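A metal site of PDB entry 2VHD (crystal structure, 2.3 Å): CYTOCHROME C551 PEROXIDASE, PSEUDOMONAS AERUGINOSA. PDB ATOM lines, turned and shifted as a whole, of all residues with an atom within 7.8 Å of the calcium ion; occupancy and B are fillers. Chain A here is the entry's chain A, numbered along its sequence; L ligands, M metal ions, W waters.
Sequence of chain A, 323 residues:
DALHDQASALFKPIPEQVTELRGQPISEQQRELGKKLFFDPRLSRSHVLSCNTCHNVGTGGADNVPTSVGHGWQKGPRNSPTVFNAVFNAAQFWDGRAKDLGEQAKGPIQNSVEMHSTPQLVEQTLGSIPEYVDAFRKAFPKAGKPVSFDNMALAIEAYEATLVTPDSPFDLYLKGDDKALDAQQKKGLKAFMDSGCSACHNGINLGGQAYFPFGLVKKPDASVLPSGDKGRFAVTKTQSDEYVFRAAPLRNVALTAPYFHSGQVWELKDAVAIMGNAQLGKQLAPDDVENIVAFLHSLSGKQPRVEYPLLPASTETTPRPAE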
ATOM      1  N   ALA A  62      33.714  10.110  -1.264  1.00  0.00           N
ATOM      2  CA  ALA A  62      33.330   9.625  -2.577  1.00  0.00           C
ATOM      3  C   ALA A  62      34.534   9.815  -3.484  1.00  0.00           C
ATOM      4  O   ALA A  62      35.446  10.559  -3.136  1.00  0.00           O
ATOM      5  CB  ALA A  62      32.126  10.411  -3.129  1.00  0.00           C
ATOM      6  N   ASP A  63      34.527   9.212  -4.679  1.00  0.00           N
ATOM      7  CA  ASP A  63      35.710   9.339  -5.562  1.00  0.00           C
ATOM      8  C   ASP A  63      35.526  10.505  -6.538  1.00  0.00           C
ATOM      9  O   ASP A  63      36.490  10.922  -7.188  1.00  0.00           O
ATOM     10  CB  ASP A  63      36.033   8.022  -6.307  1.00  0.00           C
ATOM     11  CG  ASP A  63      34.847   7.497  -7.119  1.00  0.00           C
ATOM     12  OD1 ASP A  63      33.864   8.247  -7.319  1.00  0.00           O
ATOM     13  OD2 ASP A  63      34.883   6.337  -7.570  1.00  0.00           O
ATOM     14  N   ASN A  64      34.273  11.010  -6.644  1.00  0.00           N
ATOM     15  CA  ASN A  64      33.947  12.244  -7.399  1.00  0.00           C
ATOM     16  C   ASN A  64      34.313  12.148  -8.904  1.00  0.00           C
ATOM     17  O   ASN A  64      34.874  13.058  -9.503  1.00  0.00           O
ATOM     18  CB  ASN A  64      34.612  13.462  -6.731  1.00  0.00           C
ATOM     19  CG  ASN A  64      33.996  13.769  -5.404  1.00  0.00           C
ATOM     20  OD1 ASN A  64      32.936  13.255  -5.081  1.00  0.00           O
ATOM     21  ND2 ASN A  64      34.655  14.601  -4.606  1.00  0.00           N
ATOM     22  N   VAL A  65      33.957  11.021  -9.476  1.00  0.00           N
ATOM     23  CA  VAL A  65      34.200  10.679 -10.858  1.00  0.00           C
ATOM     24  C   VAL A  65      32.796  10.193 -11.250  1.00  0.00           C
ATOM     25  O   VAL A  65      32.077   9.730 -10.348  1.00  0.00           O
ATOM     26  CB  VAL A  65      35.345   9.612 -10.853  1.00  0.00           C
ATOM     27  CG1 VAL A  65      35.052   8.439 -11.633  1.00  0.00           C
ATOM     28  CG2 VAL A  65      36.722  10.251 -11.205  1.00  0.00           C
ATOM     29  N   PRO A  66      32.374  10.332 -12.553  1.00  0.00           N
ATOM     30  CA  PRO A  66      30.954  10.057 -12.887  1.00  0.00           C
ATOM     31  C   PRO A  66      30.523   8.689 -12.409  1.00  0.00           C
ATOM     32  O   PRO A  66      29.580   8.597 -11.613  1.00  0.00           O
ATOM     33  CB  PRO A  66      30.904  10.180 -14.419  1.00  0.00           C
ATOM     34  CG  PRO A  66      31.961  11.192 -14.706  1.00  0.00           C
ATOM     35  CD  PRO A  66      33.106  10.792 -13.753  1.00  0.00           C
ATOM     36  N   ASN A  79      27.424   6.196  -9.875  1.00  0.00           N
ATOM     37  CA  ASN A  79      28.205   7.124  -9.054  1.00  0.00           C
ATOM     38  C   ASN A  79      28.350   6.559  -7.624  1.00  0.00           C
ATOM     39  O   ASN A  79      27.382   6.077  -7.038  1.00  0.00           O
ATOM     40  CB  ASN A  79      27.541   8.506  -9.066  1.00  0.00           C
ATOM     41  CG  ASN A  79      28.393   9.588  -8.412  1.00  0.00           C
ATOM     42  OD1 ASN A  79      28.092  10.038  -7.308  1.00  0.00           O
ATOM     43  ND2 ASN A  79      29.438  10.037  -9.112  1.00  0.00           N
ATOM     44  N   SER A  80      29.558   6.533  -7.080  1.00  0.00           N
ATOM     45  CA  SER A  80      29.687   5.982  -5.718  1.00  0.00           C
ATOM     46  C   SER A  80      29.326   7.026  -4.688  1.00  0.00           C
ATOM     47  O   SER A  80      29.889   8.113  -4.706  1.00  0.00           O
ATOM     48  CB  SER A  80      31.044   5.320  -5.440  1.00  0.00           C
ATOM     49  OG  SER A  80      32.062   6.230  -5.173  1.00  0.00           O
ATOM     50  N   PRO A  81      28.391   6.674  -3.773  1.00  0.00           N
ATOM     51  CA  PRO A  81      27.973   7.647  -2.817  1.00  0.00           C
ATOM     52  C   PRO A  81      29.022   7.779  -1.682  1.00  0.00           C
ATOM     53  O   PRO A  81      29.950   6.995  -1.596  1.00  0.00           O
ATOM     54  CB  PRO A  81      26.618   7.091  -2.298  1.00  0.00           C
ATOM     55  CG  PRO A  81      26.421   5.779  -3.003  1.00  0.00           C
ATOM     56  CD  PRO A  81      27.746   5.390  -3.505  1.00  0.00           C
ATOM     57  N   THR A  82      28.862   8.756  -0.806  1.00  0.00           N
ATOM     58  CA  THR A  82      29.797   8.868   0.292  1.00  0.00           C
ATOM     59  C   THR A  82      29.478   7.775   1.308  1.00  0.00           C
ATOM     60  O   THR A  82      28.315   7.384   1.508  1.00  0.00           O
ATOM     61  CB  THR A  82      29.774  10.267   0.929  1.00  0.00           C
ATOM     62  OG1 THR A  82      30.660  10.294   2.039  1.00  0.00           O
ATOM     63  CG2 THR A  82      28.359  10.662   1.434  1.00  0.00           C
ATOM     64  N   TRP A  94      22.219   2.685  -3.971  1.00  0.00           N
ATOM     65  CA  TRP A  94      21.195   3.444  -4.672  1.00  0.00           C
ATOM     66  C   TRP A  94      19.832   2.732  -4.765  1.00  0.00           C
ATOM     67  O   TRP A  94      18.784   3.399  -4.924  1.00  0.00           O
ATOM     68  CB  TRP A  94      21.663   3.845  -6.082  1.00  0.00           C
ATOM     69  CG  TRP A  94      22.730   4.915  -6.129  1.00  0.00           C
ATOM     70  CD1 TRP A  94      24.079   4.734  -6.285  1.00  0.00           C
ATOM     71  CD2 TRP A  94      22.529   6.338  -6.010  1.00  0.00           C
ATOM     72  NE1 TRP A  94      24.709   5.944  -6.280  1.00  0.00           N
ATOM     73  CE2 TRP A  94      23.797   6.947  -6.090  1.00  0.00           C
ATOM     74  CE3 TRP A  94      21.386   7.157  -5.840  1.00  0.00           C
ATOM     75  CZ2 TRP A  94      23.970   8.340  -6.019  1.00  0.00           C
ATOM     76  CZ3 TRP A  94      21.568   8.550  -5.784  1.00  0.00           C
ATOM     77  CH2 TRP A  94      22.846   9.120  -5.877  1.00  0.00           C
ATOM     78  N   ASN A 252      26.745  16.619   3.104  1.00  0.00           N
ATOM     79  CA  ASN A 252      27.971  16.756   2.351  1.00  0.00           C
ATOM     80  C   ASN A 252      27.800  16.697   0.822  1.00  0.00           C
ATOM     81  O   ASN A 252      28.746  16.393   0.110  1.00  0.00           O
ATOM     82  CB  ASN A 252      28.973  15.714   2.831  1.00  0.00           C
ATOM     83  CG  ASN A 252      29.243  15.788   4.334  1.00  0.00           C
ATOM     84  OD1 ASN A 252      29.711  16.820   4.862  1.00  0.00           O
ATOM     85  ND2 ASN A 252      28.998  14.685   5.028  1.00  0.00           N
ATOM     86  N   VAL A 253      26.599  17.034   0.330  1.00  0.00           N
ATOM     87  CA  VAL A 253      26.295  17.063  -1.119  1.00  0.00           C
ATOM     88  C   VAL A 253      27.158  18.080  -1.886  1.00  0.00           C
ATOM     89  O   VAL A 253      27.489  17.857  -3.052  1.00  0.00           O
ATOM     90  CB  VAL A 253      24.803  17.329  -1.358  1.00  0.00           C
ATOM     91  CG1 VAL A 253      24.416  18.754  -0.853  1.00  0.00           C
ATOM     92  CG2 VAL A 253      24.397  17.065  -2.861  1.00  0.00           C
ATOM     93  N   LEU A 255      30.230  18.414  -1.486  1.00  0.00           N
ATOM     94  CA  LEU A 255      31.590  17.848  -1.555  1.00  0.00           C
ATOM     95  C   LEU A 255      31.755  16.637  -2.474  1.00  0.00           C
ATOM     96  O   LEU A 255      32.872  16.141  -2.676  1.00  0.00           O
ATOM     97  CB  LEU A 255      32.097  17.485  -0.159  1.00  0.00           C
ATOM     98  CG  LEU A 255      31.994  18.569   0.928  1.00  0.00           C
ATOM     99  CD1 LEU A 255      32.459  17.956   2.202  1.00  0.00           C
ATOM    100  CD2 LEU A 255      32.789  19.833   0.579  1.00  0.00           C
ATOM    101  N   THR A 256      30.626  16.194  -3.054  1.00  0.00           N
ATOM    102  CA  THR A 256      30.516  14.921  -3.732  1.00  0.00           C
ATOM    103  C   THR A 256      29.946  15.033  -5.169  1.00  0.00           C
ATOM    104  O   THR A 256      29.284  14.097  -5.652  1.00  0.00           O
ATOM    105  CB  THR A 256      29.638  13.930  -2.876  1.00  0.00           C
ATOM    106  OG1 THR A 256      28.315  14.453  -2.724  1.00  0.00           O
ATOM    107  CG2 THR A 256      30.242  13.728  -1.474  1.00  0.00           C
ATOM    108  N   ALA A 257      30.165  16.152  -5.858  1.00  0.00           N
ATOM    109  CA  ALA A 257      29.838  16.216  -7.289  1.00  0.00           C
ATOM    110  C   ALA A 257      30.666  15.165  -8.019  1.00  0.00           C
ATOM    111  O   ALA A 257      31.803  14.914  -7.641  1.00  0.00           O
ATOM    112  CB  ALA A 257      30.114  17.614  -7.876  1.00  0.00           C
ATOM    113  N   PRO A 258      30.124  14.582  -9.103  1.00  0.00           N
ATOM    114  CA  PRO A 258      28.844  14.826  -9.720  1.00  0.00           C
ATOM    115  C   PRO A 258      27.636  14.153  -9.052  1.00  0.00           C
ATOM    116  O   PRO A 258      27.807  13.326  -8.155  1.00  0.00           O
ATOM    117  CB  PRO A 258      29.043  14.309 -11.149  1.00  0.00           C
ATOM    118  CG  PRO A 258      30.060  13.247 -11.031  1.00  0.00           C
ATOM    119  CD  PRO A 258      30.917  13.581  -9.862  1.00  0.00           C
ATOM    120  N   TYR A 259      26.429  14.442  -9.544  1.00  0.00           N
ATOM    121  CA  TYR A 259      25.212  14.087  -8.867  1.00  0.00           C
ATOM    122  C   TYR A 259      24.295  13.083  -9.548  1.00  0.00           C
ATOM    123  O   TYR A 259      24.468  12.759 -10.731  1.00  0.00           O
ATOM    124  CB  TYR A 259      24.456  15.362  -8.533  1.00  0.00           C
ATOM    125  CG  TYR A 259      25.343  16.278  -7.732  1.00  0.00           C
ATOM    126  CD1 TYR A 259      25.691  15.938  -6.439  1.00  0.00           C
ATOM    127  CD2 TYR A 259      25.867  17.472  -8.294  1.00  0.00           C
ATOM    128  CE1 TYR A 259      26.534  16.773  -5.677  1.00  0.00           C
ATOM    129  CE2 TYR A 259      26.711  18.311  -7.545  1.00  0.00           C
ATOM    130  CZ  TYR A 259      27.030  17.953  -6.221  1.00  0.00           C
ATOM    131  OH  TYR A 259      27.822  18.757  -5.446  1.00  0.00           O
ATOM    132  N   PHE A 260      23.320  12.604  -8.761  1.00  0.00           N
ATOM    133  CA  PHE A 260      22.492  11.431  -9.058  1.00  0.00           C
ATOM    134  C   PHE A 260      23.305  10.144  -9.247  1.00  0.00           C
ATOM    135  O   PHE A 260      24.563  10.182  -9.268  1.00  0.00           O
ATOM    136  CB  PHE A 260      21.525  11.706 -10.236  1.00  0.00           C
ATOM    137  CG  PHE A 260      20.872  13.028 -10.133  1.00  0.00           C
ATOM    138  CD1 PHE A 260      20.015  13.311  -9.065  1.00  0.00           C
ATOM    139  CD2 PHE A 260      21.169  14.041 -11.070  1.00  0.00           C
ATOM    140  CE1 PHE A 260      19.443  14.550  -8.951  1.00  0.00           C
ATOM    141  CE2 PHE A 260      20.614  15.295 -10.981  1.00  0.00           C
ATOM    142  CZ  PHE A 260      19.746  15.563  -9.925  1.00  0.00           C
ATOM    143  N   HIS A 261      22.578   9.020  -9.351  1.00  0.00           N
ATOM    144  CA  HIS A 261      23.223   7.702  -9.394  1.00  0.00           C
ATOM    145  C   HIS A 261      24.101   7.582 -10.611  1.00  0.00           C
ATOM    146  O   HIS A 261      25.063   6.803 -10.613  1.00  0.00           O
ATOM    147  CB  HIS A 261      22.191   6.569  -9.337  1.00  0.00           C
ATOM    148  CG  HIS A 261      21.300   6.507 -10.547  1.00  0.00           C
ATOM    149  ND1 HIS A 261      20.111   7.189 -10.627  1.00  0.00           N
ATOM    150  CD2 HIS A 261      21.427   5.823 -11.708  1.00  0.00           C
ATOM    151  CE1 HIS A 261      19.540   6.938 -11.792  1.00  0.00           C
ATOM    152  NE2 HIS A 261      20.326   6.118 -12.473  1.00  0.00           N
ATOM    153  N   GLY A 263      25.964  10.044 -12.152  1.00  0.00           N
ATOM    154  CA  GLY A 263      27.125  10.951 -12.124  1.00  0.00           C
ATOM    155  C   GLY A 263      27.309  11.871 -13.311  1.00  0.00           C
ATOM    156  O   GLY A 263      28.448  12.164 -13.705  1.00  0.00           O
ATOM    157  N   VAL A 265      25.718  14.970 -13.852  1.00  0.00           N
ATOM    158  CA  VAL A 265      25.413  16.354 -13.530  1.00  0.00           C
ATOM    159  C   VAL A 265      26.491  16.894 -12.594  1.00  0.00           C
ATOM    160  O   VAL A 265      26.595  16.488 -11.447  1.00  0.00           O
ATOM    161  CB  VAL A 265      23.965  16.444 -12.928  1.00  0.00           C
ATOM    162  CG1 VAL A 265      23.636  17.808 -12.294  1.00  0.00           C
ATOM    163  CG2 VAL A 265      22.949  16.157 -14.022  1.00  0.00           C
HETATM  164 FE1  LIG L   1      15.854  14.951  -4.483  1.00  0.00          FE
HETATM  165  C1  LIG L   1      18.553  13.098  -5.454  1.00  0.00           C
HETATM  166  C2  LIG L   1      17.892  17.750  -4.297  1.00  0.00           C
HETATM  167  C3  LIG L   1      13.071  17.015  -4.128  1.00  0.00           C
HETATM  168  C4  LIG L   1      13.868  12.277  -4.112  1.00  0.00           C
HETATM  169  N1  LIG L   1      17.893  15.366  -4.811  1.00  0.00           N
HETATM  170  C5  LIG L   1      18.841  14.440  -5.236  1.00  0.00           C
HETATM  171  C6  LIG L   1      20.121  15.154  -5.401  1.00  0.00           C
HETATM  172  C7  LIG L   1      19.908  16.429  -5.062  1.00  0.00           C
HETATM  173  C8  LIG L   1      18.516  16.585  -4.677  1.00  0.00           C
HETATM  174  C9  LIG L   1      20.930  17.566  -5.059  1.00  0.00           C
HETATM  175  C10 LIG L   1      21.483  14.575  -5.852  1.00  0.00           C
HETATM  176  C11 LIG L   1      22.109  13.875  -4.636  1.00  0.00           C
HETATM  177  C12 LIG L   1      23.372  13.137  -4.928  1.00  0.00           C
HETATM  178  O1  LIG L   1      24.042  12.820  -3.940  1.00  0.00           O
HETATM  179  O2  LIG L   1      23.752  12.836  -6.083  1.00  0.00           O
HETATM  180  N2  LIG L   1      15.565  16.979  -4.242  1.00  0.00           N
HETATM  181  C13 LIG L   1      16.522  17.955  -4.259  1.00  0.00           C
HETATM  182  C14 LIG L   1      15.855  19.247  -4.254  1.00  0.00           C
HETATM  183  C15 LIG L   1      14.509  19.030  -4.199  1.00  0.00           C
HETATM  184  C16 LIG L   1      14.308  17.611  -4.212  1.00  0.00           C
HETATM  185  C17 LIG L   1      16.624  20.602  -4.219  1.00  0.00           C
HETATM  186  C18 LIG L   1      13.317  20.036  -4.134  1.00  0.00           C
HETATM  187  C19 LIG L   1      13.473  21.189  -5.138  1.00  0.00           C
HETATM  188  N3  LIG L   1      13.822  14.719  -4.142  1.00  0.00           N
HETATM  189  C20 LIG L   1      12.833  15.670  -4.073  1.00  0.00           C
HETATM  190  C21 LIG L   1      11.558  14.991  -3.866  1.00  0.00           C
HETATM  191  C22 LIG L   1      11.788  13.655  -3.987  1.00  0.00           C
HETATM  192  C23 LIG L   1      13.209  13.478  -4.084  1.00  0.00           C
HETATM  193  C24 LIG L   1      10.205  15.753  -3.884  1.00  0.00           C
HETATM  194  C25 LIG L   1      10.851  12.426  -3.872  1.00  0.00           C
HETATM  195  C26 LIG L   1       9.522  12.471  -4.617  1.00  0.00           C
HETATM  196  N4  LIG L   1      16.185  12.971  -4.657  1.00  0.00           N
HETATM  197  C27 LIG L   1      15.129  12.059  -4.613  1.00  0.00           C
HETATM  198  C28 LIG L   1      15.568  10.822  -5.185  1.00  0.00           C
HETATM  199  C29 LIG L   1      17.029  11.066  -5.594  1.00  0.00           C
HETATM  200  C30 LIG L   1      17.338  12.441  -5.248  1.00  0.00           C
HETATM  201  C31 LIG L   1      14.746   9.516  -5.346  1.00  0.00           C
HETATM  202  C32 LIG L   1      17.929  10.019  -6.264  1.00  0.00           C
HETATM  203  C33 LIG L   1      17.671  10.121  -7.765  1.00  0.00           C
HETATM  204  C34 LIG L   1      18.739   9.310  -8.480  1.00  0.00           C
HETATM  205  O3  LIG L   1      19.926   9.763  -8.564  1.00  0.00           O
HETATM  206  O4  LIG L   1      18.385   8.199  -8.966  1.00  0.00           O
HETATM  207 CA    CA M   1      28.236  12.158  -6.254  1.00  0.00          CA
HETATM  208  O   HOH W   1      26.677  13.174  -4.600  1.00  0.00           O
HETATM  209  O   HOH W   2      28.594  10.863  -4.385  1.00  0.00           O
HETATM  210  O   HOH W   3      25.769  11.352  -6.521  1.00  0.00           O
HETATM  211  O   HOH W   4      30.609  11.696  -6.909  1.00  0.00           O
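O2 of the ligand is in hydrogen-bond range of N of Phe 260. O4 of the ligand is in hydrogen-bond range of ND1 of His 261, at 2.6 Å. The backbone NH of His 261 sits at hydrogen-bond distance from an oxygen (O3) of the ligand (2.9 Å).
The calcium ion is bound by the backbone carbonyl oxygen (O) of Pro 258 (2.3 Å), the backbone carbonyl oxygen (O) of Thr 256 (2.3 Å), water W2 (2.3 Å), the side-chain amide oxygen (OD1) of Asn 79 (2.4 Å), water W1 (2.5 Å), water W4 (2.5 Å) and water W3 (2.6 Å).
O of Pro 66 lies within hydrogen-bond range of ND2 of Asn 79, 2.9 Å away. N of Asn 79 is in hydrogen-bond range of O of His 261, 2.5 Å away. The side-chain hydroxyl of Thr 256 lies close to the backbone carbonyl oxygen of Asn 252, at 3.5 Å. ND2 of Asn 79 is in hydrogen-bond range of O of Val 65. O of Asn 79 is in hydrogen-bond range of NE1 of Trp 94 (2.8 Å).
Water W4 bridges the side-chain amide nitrogen (ND2) of Asn 79 (3.0 Å) and the side-chain amide oxygen (OD1) of Asn 64 (3.3 Å). Water W3 lies within hydrogen-bond range of an oxygen (O2) of the ligand (2.5 Å) and the backbone carbonyl oxygen of Phe 260 (3.2 Å). Water W1 lies within hydrogen-bond range of an oxygen (O1) of the ligand (2.7 Å) and the side-chain hydroxyl (OG1) of Thr 256 (2.8 Å).
The nearest printed residue that does not touch the calcium ion is Ala 257 (4.2 Å).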
